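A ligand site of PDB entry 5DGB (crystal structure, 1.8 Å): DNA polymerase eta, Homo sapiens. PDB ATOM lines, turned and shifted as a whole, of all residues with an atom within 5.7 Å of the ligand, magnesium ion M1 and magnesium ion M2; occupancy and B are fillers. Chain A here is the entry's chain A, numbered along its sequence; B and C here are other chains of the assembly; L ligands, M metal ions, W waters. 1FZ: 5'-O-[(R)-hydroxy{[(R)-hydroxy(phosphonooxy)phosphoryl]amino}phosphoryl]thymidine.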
ATOM      1  N   ASP A  16      -9.599  12.757 -26.182  1.00  0.00           N
ATOM      2  CA  ASP A  16      -9.916  14.167 -25.932  1.00  0.00           C
ATOM      3  C   ASP A  16      -8.947  14.814 -24.928  1.00  0.00           C
ATOM      4  O   ASP A  16      -8.806  14.335 -23.810  1.00  0.00           O
ATOM      5  CB  ASP A  16     -11.341  14.324 -25.421  1.00  0.00           C
ATOM      6  CG  ASP A  16     -11.764  15.771 -25.339  1.00  0.00           C
ATOM      7  OD1 ASP A  16     -11.353  16.440 -24.378  1.00  0.00           O
ATOM      8  OD2 ASP A  16     -12.479  16.233 -26.239  1.00  0.00           O
ATOM      9  N   MET A  17      -8.330  15.911 -25.326  1.00  0.00           N
ATOM     10  CA  MET A  17      -7.366  16.587 -24.455  1.00  0.00           C
ATOM     11  C   MET A  17      -8.035  17.157 -23.191  1.00  0.00           C
ATOM     12  O   MET A  17      -9.132  17.702 -23.247  1.00  0.00           O
ATOM     13  CB  MET A  17      -6.639  17.714 -25.217  1.00  0.00           C
ATOM     14  CG  MET A  17      -6.007  17.299 -26.561  1.00  0.00           C
ATOM     15  SD  MET A  17      -4.887  15.882 -26.430  1.00  0.00           S
ATOM     16  CE  MET A  17      -3.655  16.474 -25.331  1.00  0.00           C
ATOM     17  N   ASP A  18      -7.365  17.002 -22.056  1.00  0.00           N
ATOM     18  CA  ASP A  18      -7.865  17.591 -20.814  1.00  0.00           C
ATOM     19  C   ASP A  18      -7.624  19.096 -20.810  1.00  0.00           C
ATOM     20  O   ASP A  18      -6.541  19.528 -21.178  1.00  0.00           O
ATOM     21  CB  ASP A  18      -7.181  16.947 -19.609  1.00  0.00           C
ATOM     22  CG  ASP A  18      -7.409  15.439 -19.539  1.00  0.00           C
ATOM     23  OD1 ASP A  18      -8.444  14.967 -20.047  1.00  0.00           O
ATOM     24  OD2 ASP A  18      -6.568  14.734 -18.945  1.00  0.00           O
ATOM     25  N   CYS A  19      -8.632  19.844 -20.356  1.00  0.00           N
ATOM     26  CA  CYS A  19      -8.646  21.315 -20.352  1.00  0.00           C
ATOM     27  C   CYS A  19      -7.642  21.912 -21.335  1.00  0.00           C
ATOM     28  O   CYS A  19      -6.660  22.540 -20.958  1.00  0.00           O
ATOM     29  CB  CYS A  19      -8.406  21.853 -18.925  1.00  0.00           C
ATOM     30  SG  CYS A  19      -6.949  21.190 -18.022  1.00  0.00           S
ATOM     31  N   PHE A  20      -7.897  21.702 -22.621  1.00  0.00           N
ATOM     32  CA  PHE A  20      -6.852  21.822 -23.639  1.00  0.00           C
ATOM     33  C   PHE A  20      -6.181  23.187 -23.705  1.00  0.00           C
ATOM     34  O   PHE A  20      -4.959  23.274 -23.574  1.00  0.00           O
ATOM     35  CB  PHE A  20      -7.417  21.478 -25.022  1.00  0.00           C
ATOM     36  CG  PHE A  20      -6.372  21.447 -26.100  1.00  0.00           C
ATOM     37  CD1 PHE A  20      -5.139  20.854 -25.861  1.00  0.00           C
ATOM     38  CD2 PHE A  20      -6.624  22.008 -27.345  1.00  0.00           C
ATOM     39  CE1 PHE A  20      -4.154  20.825 -26.843  1.00  0.00           C
ATOM     40  CE2 PHE A  20      -5.632  21.973 -28.344  1.00  0.00           C
ATOM     41  CZ  PHE A  20      -4.409  21.355 -28.091  1.00  0.00           C
ATOM     42  N   PHE A  21      -6.949  24.272 -23.876  1.00  0.00           N
ATOM     43  CA  PHE A  21      -6.305  25.587 -24.052  1.00  0.00           C
ATOM     44  C   PHE A  21      -5.521  25.946 -22.781  1.00  0.00           C
ATOM     45  O   PHE A  21      -4.483  26.605 -22.870  1.00  0.00           O
ATOM     46  CB  PHE A  21      -7.300  26.711 -24.365  1.00  0.00           C
ATOM     47  CG  PHE A  21      -7.924  26.643 -25.746  1.00  0.00           C
ATOM     48  CD1 PHE A  21      -7.838  25.510 -26.538  1.00  0.00           C
ATOM     49  CD2 PHE A  21      -8.609  27.749 -26.246  1.00  0.00           C
ATOM     50  CE1 PHE A  21      -8.417  25.467 -27.806  1.00  0.00           C
ATOM     51  CE2 PHE A  21      -9.193  27.714 -27.518  1.00  0.00           C
ATOM     52  CZ  PHE A  21      -9.100  26.568 -28.292  1.00  0.00           C
ATOM     53  N   VAL A  22      -6.013  25.513 -21.621  1.00  0.00           N
ATOM     54  CA  VAL A  22      -5.295  25.725 -20.351  1.00  0.00           C
ATOM     55  C   VAL A  22      -3.946  24.988 -20.370  1.00  0.00           C
ATOM     56  O   VAL A  22      -2.914  25.570 -19.994  1.00  0.00           O
ATOM     57  CB  VAL A  22      -6.139  25.268 -19.134  1.00  0.00           C
ATOM     58  CG1 VAL A  22      -5.279  25.193 -17.860  1.00  0.00           C
ATOM     59  CG2 VAL A  22      -7.331  26.210 -18.922  1.00  0.00           C
ATOM     60  N   ILE A  51     -12.998  30.565 -21.542  1.00  0.00           N
ATOM     61  CA  ILE A  51     -13.309  29.520 -22.517  1.00  0.00           C
ATOM     62  C   ILE A  51     -12.691  28.159 -22.168  1.00  0.00           C
ATOM     63  O   ILE A  51     -13.041  27.163 -22.791  1.00  0.00           O
ATOM     64  CB  ILE A  51     -12.874  29.918 -23.937  1.00  0.00           C
ATOM     65  CG1 ILE A  51     -11.370  30.174 -24.045  1.00  0.00           C
ATOM     66  CG2 ILE A  51     -13.646  31.180 -24.405  1.00  0.00           C
ATOM     67  CD1 ILE A  51     -10.929  30.452 -25.476  1.00  0.00           C
ATOM     68  N   ALA A  52     -11.811  28.121 -21.164  1.00  0.00           N
ATOM     69  CA  ALA A  52     -11.258  26.841 -20.685  1.00  0.00           C
ATOM     70  C   ALA A  52     -10.818  26.945 -19.236  1.00  0.00           C
ATOM     71  O   ALA A  52     -10.388  28.009 -18.798  1.00  0.00           O
ATOM     72  CB  ALA A  52     -10.075  26.396 -21.583  1.00  0.00           C
ATOM     73  N   VAL A  53     -10.949  25.844 -18.483  1.00  0.00           N
ATOM     74  CA  VAL A  53     -10.789  25.861 -17.029  1.00  0.00           C
ATOM     75  C   VAL A  53     -10.002  24.654 -16.526  1.00  0.00           C
ATOM     76  O   VAL A  53     -10.346  23.510 -16.849  1.00  0.00           O
ATOM     77  CB  VAL A  53     -12.171  25.869 -16.313  1.00  0.00           C
ATOM     78  CG1 VAL A  53     -12.014  26.149 -14.830  1.00  0.00           C
ATOM     79  CG2 VAL A  53     -13.105  26.888 -16.941  1.00  0.00           C
ATOM     80  N   TYR A  55      -8.664  21.726 -13.970  1.00  0.00           N
ATOM     81  CA  TYR A  55      -9.462  20.912 -13.053  1.00  0.00           C
ATOM     82  C   TYR A  55      -9.394  21.458 -11.624  1.00  0.00           C
ATOM     83  O   TYR A  55     -10.391  21.414 -10.908  1.00  0.00           O
ATOM     84  CB  TYR A  55      -9.036  19.429 -13.135  1.00  0.00           C
ATOM     85  CG  TYR A  55      -9.693  18.804 -14.348  1.00  0.00           C
ATOM     86  CD1 TYR A  55      -9.158  18.979 -15.622  1.00  0.00           C
ATOM     87  CD2 TYR A  55     -10.886  18.108 -14.237  1.00  0.00           C
ATOM     88  CE1 TYR A  55      -9.789  18.445 -16.747  1.00  0.00           C
ATOM     89  CE2 TYR A  55     -11.525  17.579 -15.344  1.00  0.00           C
ATOM     90  CZ  TYR A  55     -10.971  17.739 -16.595  1.00  0.00           C
ATOM     91  OH  TYR A  55     -11.610  17.210 -17.702  1.00  0.00           O
ATOM     92  N   ARG A  58     -11.978  24.089 -11.542  1.00  0.00           N
ATOM     93  CA  ARG A  58     -13.328  23.522 -11.633  1.00  0.00           C
ATOM     94  C   ARG A  58     -13.862  23.146 -10.249  1.00  0.00           C
ATOM     95  O   ARG A  58     -15.071  23.197  -9.997  1.00  0.00           O
ATOM     96  CB  ARG A  58     -13.354  22.283 -12.534  1.00  0.00           C
ATOM     97  CG  ARG A  58     -13.015  22.595 -13.974  1.00  0.00           C
ATOM     98  CD  ARG A  58     -13.137  21.373 -14.898  1.00  0.00           C
ATOM     99  NE  ARG A  58     -12.458  21.643 -16.169  1.00  0.00           N
ATOM    100  CZ  ARG A  58     -12.608  20.908 -17.270  1.00  0.00           C
ATOM    101  NH1 ARG A  58     -13.413  19.849 -17.254  1.00  0.00           N
ATOM    102  NH2 ARG A  58     -11.932  21.232 -18.366  1.00  0.00           N
ATOM    103  N   ARG A  64     -16.654  27.303 -18.059  1.00  0.00           N
ATOM    104  CA  ARG A  64     -16.677  28.008 -19.333  1.00  0.00           C
ATOM    105  C   ARG A  64     -17.910  28.917 -19.399  1.00  0.00           C
ATOM    106  O   ARG A  64     -18.954  28.583 -18.850  1.00  0.00           O
ATOM    107  CB  ARG A  64     -16.670  27.002 -20.495  1.00  0.00           C
ATOM    108  CG  ARG A  64     -16.778  27.627 -21.863  1.00  0.00           C
ATOM    109  CD  ARG A  64     -16.712  26.580 -22.977  1.00  0.00           C
ATOM    110  NE  ARG A  64     -17.786  25.604 -22.897  1.00  0.00           N
ATOM    111  CZ  ARG A  64     -19.046  25.814 -23.303  1.00  0.00           C
ATOM    112  NH1 ARG A  64     -19.392  26.984 -23.820  1.00  0.00           N
ATOM    113  NH2 ARG A  64     -19.948  24.857 -23.199  1.00  0.00           N
ATOM    114  N   SER A 116     -12.819  17.793 -33.312  1.00  0.00           N
ATOM    115  CA  SER A 116     -12.788  19.144 -32.764  1.00  0.00           C
ATOM    116  C   SER A 116     -11.334  19.596 -32.742  1.00  0.00           C
ATOM    117  O   SER A 116     -10.435  18.844 -33.097  1.00  0.00           O
ATOM    118  CB  SER A 116     -13.387  19.197 -31.354  1.00  0.00           C
ATOM    119  OG  SER A 116     -12.453  18.699 -30.395  1.00  0.00           O
ATOM    120  N   ILE A 117     -11.083  20.820 -32.279  1.00  0.00           N
ATOM    121  CA  ILE A 117      -9.699  21.263 -32.095  1.00  0.00           C
ATOM    122  C   ILE A 117      -8.908  20.365 -31.123  1.00  0.00           C
ATOM    123  O   ILE A 117      -7.669  20.308 -31.204  1.00  0.00           O
ATOM    124  CB  ILE A 117      -9.651  22.742 -31.596  1.00  0.00           C
ATOM    125  CG1 ILE A 117      -8.240  23.316 -31.805  1.00  0.00           C
ATOM    126  CG2 ILE A 117     -10.085  22.849 -30.140  1.00  0.00           C
ATOM    127  CD1 ILE A 117      -8.170  24.844 -31.746  1.00  0.00           C
ATOM    128  N   ASP A 118      -9.586  19.634 -30.221  1.00  0.00           N
ATOM    129  CA  ASP A 118      -8.833  18.858 -29.220  1.00  0.00           C
ATOM    130  C   ASP A 118      -9.202  17.376 -29.128  1.00  0.00           C
ATOM    131  O   ASP A 118      -8.872  16.709 -28.147  1.00  0.00           O
ATOM    132  CB  ASP A 118      -9.000  19.490 -27.836  1.00  0.00           C
ATOM    133  CG  ASP A 118     -10.182  18.933 -27.051  1.00  0.00           C
ATOM    134  OD1 ASP A 118     -11.261  18.723 -27.626  1.00  0.00           O
ATOM    135  OD2 ASP A 118      -9.999  18.721 -25.829  1.00  0.00           O
ATOM    136  N   GLU A 119      -9.864  16.837 -30.153  1.00  0.00           N
ATOM    137  CA  GLU A 119     -10.190  15.411 -30.103  1.00  0.00           C
ATOM    138  C   GLU A 119     -10.292  14.774 -31.466  1.00  0.00           C
ATOM    139  O   GLU A 119     -10.561  15.432 -32.463  1.00  0.00           O
ATOM    140  CB  GLU A 119     -11.503  15.184 -29.350  1.00  0.00           C
ATOM    141  CG  GLU A 119     -12.747  15.577 -30.112  1.00  0.00           C
ATOM    142  CD  GLU A 119     -13.857  15.980 -29.161  1.00  0.00           C
ATOM    143  OE1 GLU A 119     -14.778  15.180 -28.939  1.00  0.00           O
ATOM    144  OE2 GLU A 119     -13.775  17.100 -28.618  1.00  0.00           O
ATOM    145  N   LYS A 227     -17.063   8.227 -27.231  1.00  0.00           N
ATOM    146  CA  LYS A 227     -17.158   9.590 -26.729  1.00  0.00           C
ATOM    147  C   LYS A 227     -17.746   9.646 -25.326  1.00  0.00           C
ATOM    148  O   LYS A 227     -17.210  10.331 -24.462  1.00  0.00           O
ATOM    149  CB  LYS A 227     -18.003  10.468 -27.673  1.00  0.00           C
ATOM    150  CG  LYS A 227     -18.275  11.868 -27.133  1.00  0.00           C
ATOM    151  CD  LYS A 227     -17.005  12.736 -27.089  1.00  0.00           C
ATOM    152  CE  LYS A 227     -17.348  14.208 -26.767  1.00  0.00           C
ATOM    153  NZ  LYS A 227     -16.155  15.113 -26.564  1.00  0.00           N
ATOM    154  N   LYS A 234     -12.501  11.399 -16.867  1.00  0.00           N
ATOM    155  CA  LYS A 234     -11.651  12.582 -16.998  1.00  0.00           C
ATOM    156  C   LYS A 234     -11.322  13.157 -15.633  1.00  0.00           C
ATOM    157  O   LYS A 234     -12.176  13.162 -14.756  1.00  0.00           O
ATOM    158  CB  LYS A 234     -12.327  13.678 -17.839  1.00  0.00           C
ATOM    159  CG  LYS A 234     -11.952  13.679 -19.292  1.00  0.00           C
ATOM    160  CD  LYS A 234     -12.597  14.820 -20.086  1.00  0.00           C
ATOM    161  CE  LYS A 234     -12.081  14.822 -21.535  1.00  0.00           C
ATOM    162  NZ  LYS A 234     -10.708  15.430 -21.635  1.00  0.00           N
ATOM    163  N   PRO A 235     -10.088  13.682 -15.456  1.00  0.00           N
ATOM    164  CA  PRO A 235      -9.000  13.800 -16.433  1.00  0.00           C
ATOM    165  C   PRO A 235      -7.935  12.698 -16.331  1.00  0.00           C
ATOM    166  O   PRO A 235      -7.893  11.927 -15.368  1.00  0.00           O
ATOM    167  CB  PRO A 235      -8.381  15.161 -16.083  1.00  0.00           C
ATOM    168  CG  PRO A 235      -8.498  15.204 -14.565  1.00  0.00           C
ATOM    169  CD  PRO A 235      -9.765  14.398 -14.209  1.00  0.00           C
ATOM    170  P    DT B   3     -24.680  37.213 -21.954  1.00  0.00           P
ATOM    171  OP1  DT B   3     -26.103  37.402 -22.302  1.00  0.00           O
ATOM    172  OP2  DT B   3     -24.295  36.841 -20.569  1.00  0.00           O
ATOM    173  O5'  DT B   3     -24.061  36.125 -22.933  1.00  0.00           O
ATOM    174  C5'  DT B   3     -22.887  35.420 -22.566  1.00  0.00           C
ATOM    175  C4'  DT B   3     -21.683  36.009 -23.271  1.00  0.00           C
ATOM    176  O4'  DT B   3     -20.508  35.205 -22.967  1.00  0.00           O
ATOM    177  C3'  DT B   3     -21.787  36.010 -24.806  1.00  0.00           C
ATOM    178  O3'  DT B   3     -21.174  37.181 -25.327  1.00  0.00           O
ATOM    179  C2'  DT B   3     -21.006  34.766 -25.181  1.00  0.00           C
ATOM    180  C1'  DT B   3     -19.879  34.857 -24.184  1.00  0.00           C
ATOM    181  N1   DT B   3     -19.150  33.588 -24.014  1.00  0.00           N
ATOM    182  C2   DT B   3     -17.790  33.603 -23.793  1.00  0.00           C
ATOM    183  O2   DT B   3     -17.137  34.626 -23.697  1.00  0.00           O
ATOM    184  N3   DT B   3     -17.225  32.361 -23.667  1.00  0.00           N
ATOM    185  C4   DT B   3     -17.874  31.132 -23.763  1.00  0.00           C
ATOM    186  O4   DT B   3     -17.283  30.075 -23.641  1.00  0.00           O
ATOM    187  C5   DT B   3     -19.299  31.209 -24.002  1.00  0.00           C
ATOM    188  C7   DT B   3     -20.116  29.953 -24.118  1.00  0.00           C
ATOM    189  C6   DT B   3     -19.860  32.408 -24.115  1.00  0.00           C
ATOM    190  P    DA B   4     -20.873  37.271 -26.914  1.00  0.00           P
ATOM    191  OP1  DA B   4     -20.631  38.692 -27.257  1.00  0.00           O
ATOM    192  OP2  DA B   4     -21.916  36.476 -27.597  1.00  0.00           O
ATOM    193  O5'  DA B   4     -19.499  36.468 -27.107  1.00  0.00           O
ATOM    194  C5'  DA B   4     -18.290  37.003 -26.619  1.00  0.00           C
ATOM    195  C4'  DA B   4     -17.120  36.465 -27.431  1.00  0.00           C
ATOM    196  O4'  DA B   4     -16.950  35.039 -27.200  1.00  0.00           O
ATOM    197  C3'  DA B   4     -17.251  36.608 -28.937  1.00  0.00           C
ATOM    198  O3'  DA B   4     -15.972  36.831 -29.467  1.00  0.00           O
ATOM    199  C2'  DA B   4     -17.813  35.249 -29.375  1.00  0.00           C
ATOM    200  C1'  DA B   4     -17.098  34.315 -28.404  1.00  0.00           C
ATOM    201  N9   DA B   4     -17.812  33.084 -28.090  1.00  0.00           N
ATOM    202  C8   DA B   4     -19.164  32.904 -27.949  1.00  0.00           C
ATOM    203  N7   DA B   4     -19.496  31.674 -27.629  1.00  0.00           N
ATOM    204  C5   DA B   4     -18.294  31.012 -27.530  1.00  0.00           C
ATOM    205  C6   DA B   4     -17.950  29.683 -27.206  1.00  0.00           C
ATOM    206  N6   DA B   4     -18.860  28.736 -26.929  1.00  0.00           N
ATOM    207  N1   DA B   4     -16.643  29.347 -27.206  1.00  0.00           N
ATOM    208  C2   DA B   4     -15.729  30.292 -27.492  1.00  0.00           C
ATOM    209  N3   DA B   4     -15.926  31.576 -27.807  1.00  0.00           N
ATOM    210  C4   DA B   4     -17.240  31.870 -27.800  1.00  0.00           C
ATOM    211  P   EDA B   5     -15.801  36.926 -31.010  1.00  0.00           P
ATOM    212  OP1 EDA B   5     -14.772  37.855 -31.243  1.00  0.00           O
ATOM    213  OP2 EDA B   5     -17.094  37.095 -31.644  1.00  0.00           O
ATOM    214  O5' EDA B   5     -15.211  35.490 -31.416  1.00  0.00           O
ATOM    215  N9  EDA B   5     -16.424  31.454 -31.675  1.00  0.00           N
ATOM    216  C4  EDA B   5     -16.798  30.282 -31.197  1.00  0.00           C
ATOM    217  N3  EDA B   5     -16.066  29.151 -30.995  1.00  0.00           N
ATOM    218  C2  EDA B   5     -16.649  28.038 -30.522  1.00  0.00           C
ATOM    219  N1  EDA B   5     -17.992  28.137 -30.240  1.00  0.00           N
ATOM    220  C6  EDA B   5     -18.710  29.235 -30.449  1.00  0.00           C
ATOM    221  C10 EDA B   5     -18.832  27.234 -29.798  1.00  0.00           C
ATOM    222  C11 EDA B   5     -20.026  27.777 -29.694  1.00  0.00           C
ATOM    223  N6  EDA B   5     -19.955  28.999 -30.080  1.00  0.00           N
ATOM    224  C5  EDA B   5     -18.109  30.384 -30.947  1.00  0.00           C
ATOM    225  N7  EDA B   5     -18.522  31.574 -31.229  1.00  0.00           N
ATOM    226  C8  EDA B   5     -17.475  32.241 -31.675  1.00  0.00           C
ATOM    227  C2' EDA B   5     -15.010  32.836 -33.119  1.00  0.00           C
ATOM    228  C5' EDA B   5     -14.030  35.051 -30.904  1.00  0.00           C
ATOM    229  C4' EDA B   5     -13.680  33.607 -31.353  1.00  0.00           C
ATOM    230  O4' EDA B   5     -14.479  32.752 -30.919  1.00  0.00           O
ATOM    231  C1' EDA B   5     -15.128  31.956 -32.094  1.00  0.00           C
ATOM    232  C3' EDA B   5     -13.710  33.525 -32.936  1.00  0.00           C
ATOM    233  O3' EDA B   5     -12.645  32.821 -33.400  1.00  0.00           O
ATOM    234  P    DA C   8     -19.568  18.618 -26.803  1.00  0.00           P
ATOM    235  OP1  DA C   8     -20.685  18.170 -25.941  1.00  0.00           O
ATOM    236  OP2  DA C   8     -18.895  19.916 -26.536  1.00  0.00           O
ATOM    237  O5'  DA C   8     -18.448  17.477 -26.813  1.00  0.00           O
HETATM  238  O2  1FZ L   1     -13.494  27.650 -27.060  1.00  0.00           O
HETATM  239  O4  1FZ L   1     -17.657  26.109 -26.283  1.00  0.00           O
HETATM  240  C4  1FZ L   1     -16.416  25.929 -26.352  1.00  0.00           C
HETATM  241  C5  1FZ L   1     -15.847  24.584 -26.062  1.00  0.00           C
HETATM  242  C6  1FZ L   1     -14.469  24.415 -26.154  1.00  0.00           C
HETATM  243  C5M 1FZ L   1     -16.765  23.436 -25.689  1.00  0.00           C
HETATM  244  N3  1FZ L   1     -15.595  26.928 -26.692  1.00  0.00           N
HETATM  245  C2  1FZ L   1     -14.274  26.725 -26.755  1.00  0.00           C
HETATM  246  N1  1FZ L   1     -13.700  25.462 -26.485  1.00  0.00           N
HETATM  247  C1' 1FZ L   1     -12.236  25.327 -26.616  1.00  0.00           C
HETATM  248  C2' 1FZ L   1     -11.518  25.469 -25.282  1.00  0.00           C
HETATM  249  C3' 1FZ L   1     -11.227  24.024 -24.894  1.00  0.00           C
HETATM  250  O3' 1FZ L   1     -10.039  23.908 -24.085  1.00  0.00           O
HETATM  251  O4' 1FZ L   1     -11.937  24.021 -27.136  1.00  0.00           O
HETATM  252  C4' 1FZ L   1     -11.068  23.322 -26.229  1.00  0.00           C
HETATM  253  C5' 1FZ L   1     -11.481  21.857 -26.172  1.00  0.00           C
HETATM  254  O5' 1FZ L   1     -12.863  21.747 -25.794  1.00  0.00           O
HETATM  255  PA  1FZ L   1     -13.396  20.609 -24.777  1.00  0.00           P
HETATM  256  O1A 1FZ L   1     -12.667  19.316 -25.038  1.00  0.00           O
HETATM  257  O2A 1FZ L   1     -14.918  20.589 -24.887  1.00  0.00           O
HETATM  258  N3A 1FZ L   1     -13.130  21.206 -23.153  1.00  0.00           N
HETATM  259  PB  1FZ L   1     -11.529  21.080 -22.444  1.00  0.00           P
HETATM  260  O1B 1FZ L   1     -11.103  22.466 -22.060  1.00  0.00           O
HETATM  261  O2B 1FZ L   1     -10.592  20.280 -23.318  1.00  0.00           O
HETATM  262  O3B 1FZ L   1     -11.755  20.286 -21.062  1.00  0.00           O
HETATM  263  PG  1FZ L   1     -12.111  18.721 -20.920  1.00  0.00           P
HETATM  264  O1G 1FZ L   1     -13.462  18.670 -20.254  1.00  0.00           O
HETATM  265  O3G 1FZ L   1     -12.117  18.153 -22.317  1.00  0.00           O
HETATM  266  O2G 1FZ L   1     -10.996  18.168 -20.059  1.00  0.00           O
HETATM  267 MG    MG M   1     -11.024  18.386 -24.051  1.00  0.00          MG
HETATM  268 MG    MG M   2     -13.088  18.124 -26.850  1.00  0.00          MG
HETATM  269  O   HOH W   1     -14.496  16.887 -23.246  1.00  0.00           O
HETATM  270  O   HOH W   2     -13.992  24.344 -22.446  1.00  0.00           O
HETATM  271  O   HOH W   3     -13.482  22.198 -28.970  1.00  0.00           O
HETATM  272  O   HOH W   4     -16.684  20.167 -22.585  1.00  0.00           O
HETATM  273  O   HOH W   5     -15.442  20.453 -20.257  1.00  0.00           O
HETATM  274  O   HOH W   6     -13.403  25.013 -29.756  1.00  0.00           O
HETATM  275  O   HOH W   7     -12.089  28.782 -28.978  1.00  0.00           O
HETATM  276  O   HOH W   8     -16.029  17.373 -21.378  1.00  0.00           O
HETATM  277  O   HOH W   9     -19.317  24.159 -28.143  1.00  0.00           O
HETATM  278  O   HOH W  10     -14.095  19.853 -27.867  1.00  0.00           O
HETATM  279  O   HOH W  11     -12.082  23.719 -20.037  1.00  0.00           O
HETATM  280  O   HOH W  12     -15.042  17.736 -25.825  1.00  0.00           O
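O1G of the ligand lies within salt-bridge range of NH1 of Arg 58, 3.2 Å away.
An oxygen (O2G) of the ligand lies within hydrogen-bond range of the backbone NH (N) of Cys 19, at 2.9 Å.
O2G of the ligand sits at hydrogen-bond distance from OH of Tyr 55.
The backbone NH (N) of Phe 20 is in hydrogen-bond range of an oxygen (O1B) of the ligand (3.3 Å).
N1 of DA 4 of chain B is in hydrogen-bond range of N3 of the ligand (2.7 Å).
The guanidinium group (NH1) of Arg 64 lies within hydrogen-bond range of an oxygen (O4) of the ligand (3.1 Å).
An oxygen (O3') of the ligand is in hydrogen-bond range of the backbone NH (N) of Phe 21 (3.1 Å).
The side-chain amino group (NZ) of Lys 234 lies within salt-bridge range of an oxygen (O2G) of the ligand (3.2 Å).
The side-chain carboxylate (OD2) of Asp 16 lies close to the side-chain amino group (NZ) of Lys 227, 3.9 Å away.
The backbone NH (N) of Asp 118 is in hydrogen-bond range of the side-chain hydroxyl (OG) of Ser 116 (3.0 Å).
The backbone NH (N) of Glu 119 sits close to the side-chain hydroxyl (OG) of Ser 116 (3.2 Å).
OH of Tyr 55 sits at hydrogen-bond distance from NH1 of Arg 58, 3.2 Å away.
The side-chain amino group (NZ) of Lys 234 is in salt-bridge range of the side-chain carboxylate (OD1) of Asp 18 (2.8 Å).
The backbone carbonyl oxygen (O) of Asp 16 sits at hydrogen-bond distance from the side-chain amino group (NZ) of Lys 234 (3.1 Å).
OE1 of Glu 119 is in salt-bridge range of NZ of Lys 227.
The guanidinium group (NE) of Arg 58 sits at hydrogen-bond distance from the backbone carbonyl oxygen (O) of Val 53 (2.9 Å).
Asp 18 touches the ligand (CA to O2G, 3.3 Å).
O of Ile 51 touches C2' of the ligand (3.4 Å).
Ala 52 touches the ligand.
CG2 of Ile 117 touches O4' of the ligand, at 3.7 Å.
EDA 5 of chain B touches the ligand (C10 to O4, 3.9 Å).
Hydrophobic or aromatic side chains within 4 Å of the ligand: Phe 20, Phe 21, Ile 51, Ala 52, Tyr 55 and Ile 117.
16 residues have an atom within 4 Å of the ligand: Asp 16, Met 17, Asp 18, Cys 19, Phe 20, Phe 21, Ile 51, Ala 52, Tyr 55, Arg 58, Arg 64, Ile 117, Asp 118, Lys 234, DA 4 of chain B and EDA 5 of chain B.
Lys 234 touches magnesium ion M1.
Of the 24 residues printed, 4 come within 4 Å of magnesium ion M1.
Ser 116 touches magnesium ion M2 (OG to MG, 3.6 Å).
Within 4 Å of magnesium ion M2: Asp 16, Ser 116, Asp 118 and Glu 119.
Magnesium ion M1 is bound by the side-chain carboxylate (OD1) of Asp 16, an oxygen (O3G) of the ligand, an oxygen (O2B) of the ligand, the side-chain carboxylate (OD2) of Asp 118, an oxygen (O1A) of the ligand and the backbone carbonyl oxygen (O) of Met 17.
Magnesium ion M1 has six donor atoms within binding distance.
Magnesium ion M2 is bound by the side-chain carboxylate of Asp 118 (2.1 Å), the side-chain carboxylate of Asp 16 (2.1 Å), the side-chain carboxylate of Glu 119 (2.2 Å), an oxygen (O1A) of the ligand (2.2 Å), water W12 (2.2 Å) and water W10 (2.2 Å).
Water W10 bridges an oxygen (O5') of the ligand (3.1 Å) and the side-chain hydroxyl (OG) of Ser 116 (3.2 Å).
Water W12 bridges the side-chain amino group of Lys 227 and an oxygen (O2A) of the ligand.
Water W11 lies within hydrogen-bond range of an oxygen (O1B) of the ligand, the backbone NH (N) of Val 53 and the guanidinium group (NH2) of Arg 58.
Water W2 bridges the backbone carbonyl oxygen (O) of Ile 51 (3.0 Å) and a nitrogen (N3A) of the ligand (3.3 Å).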
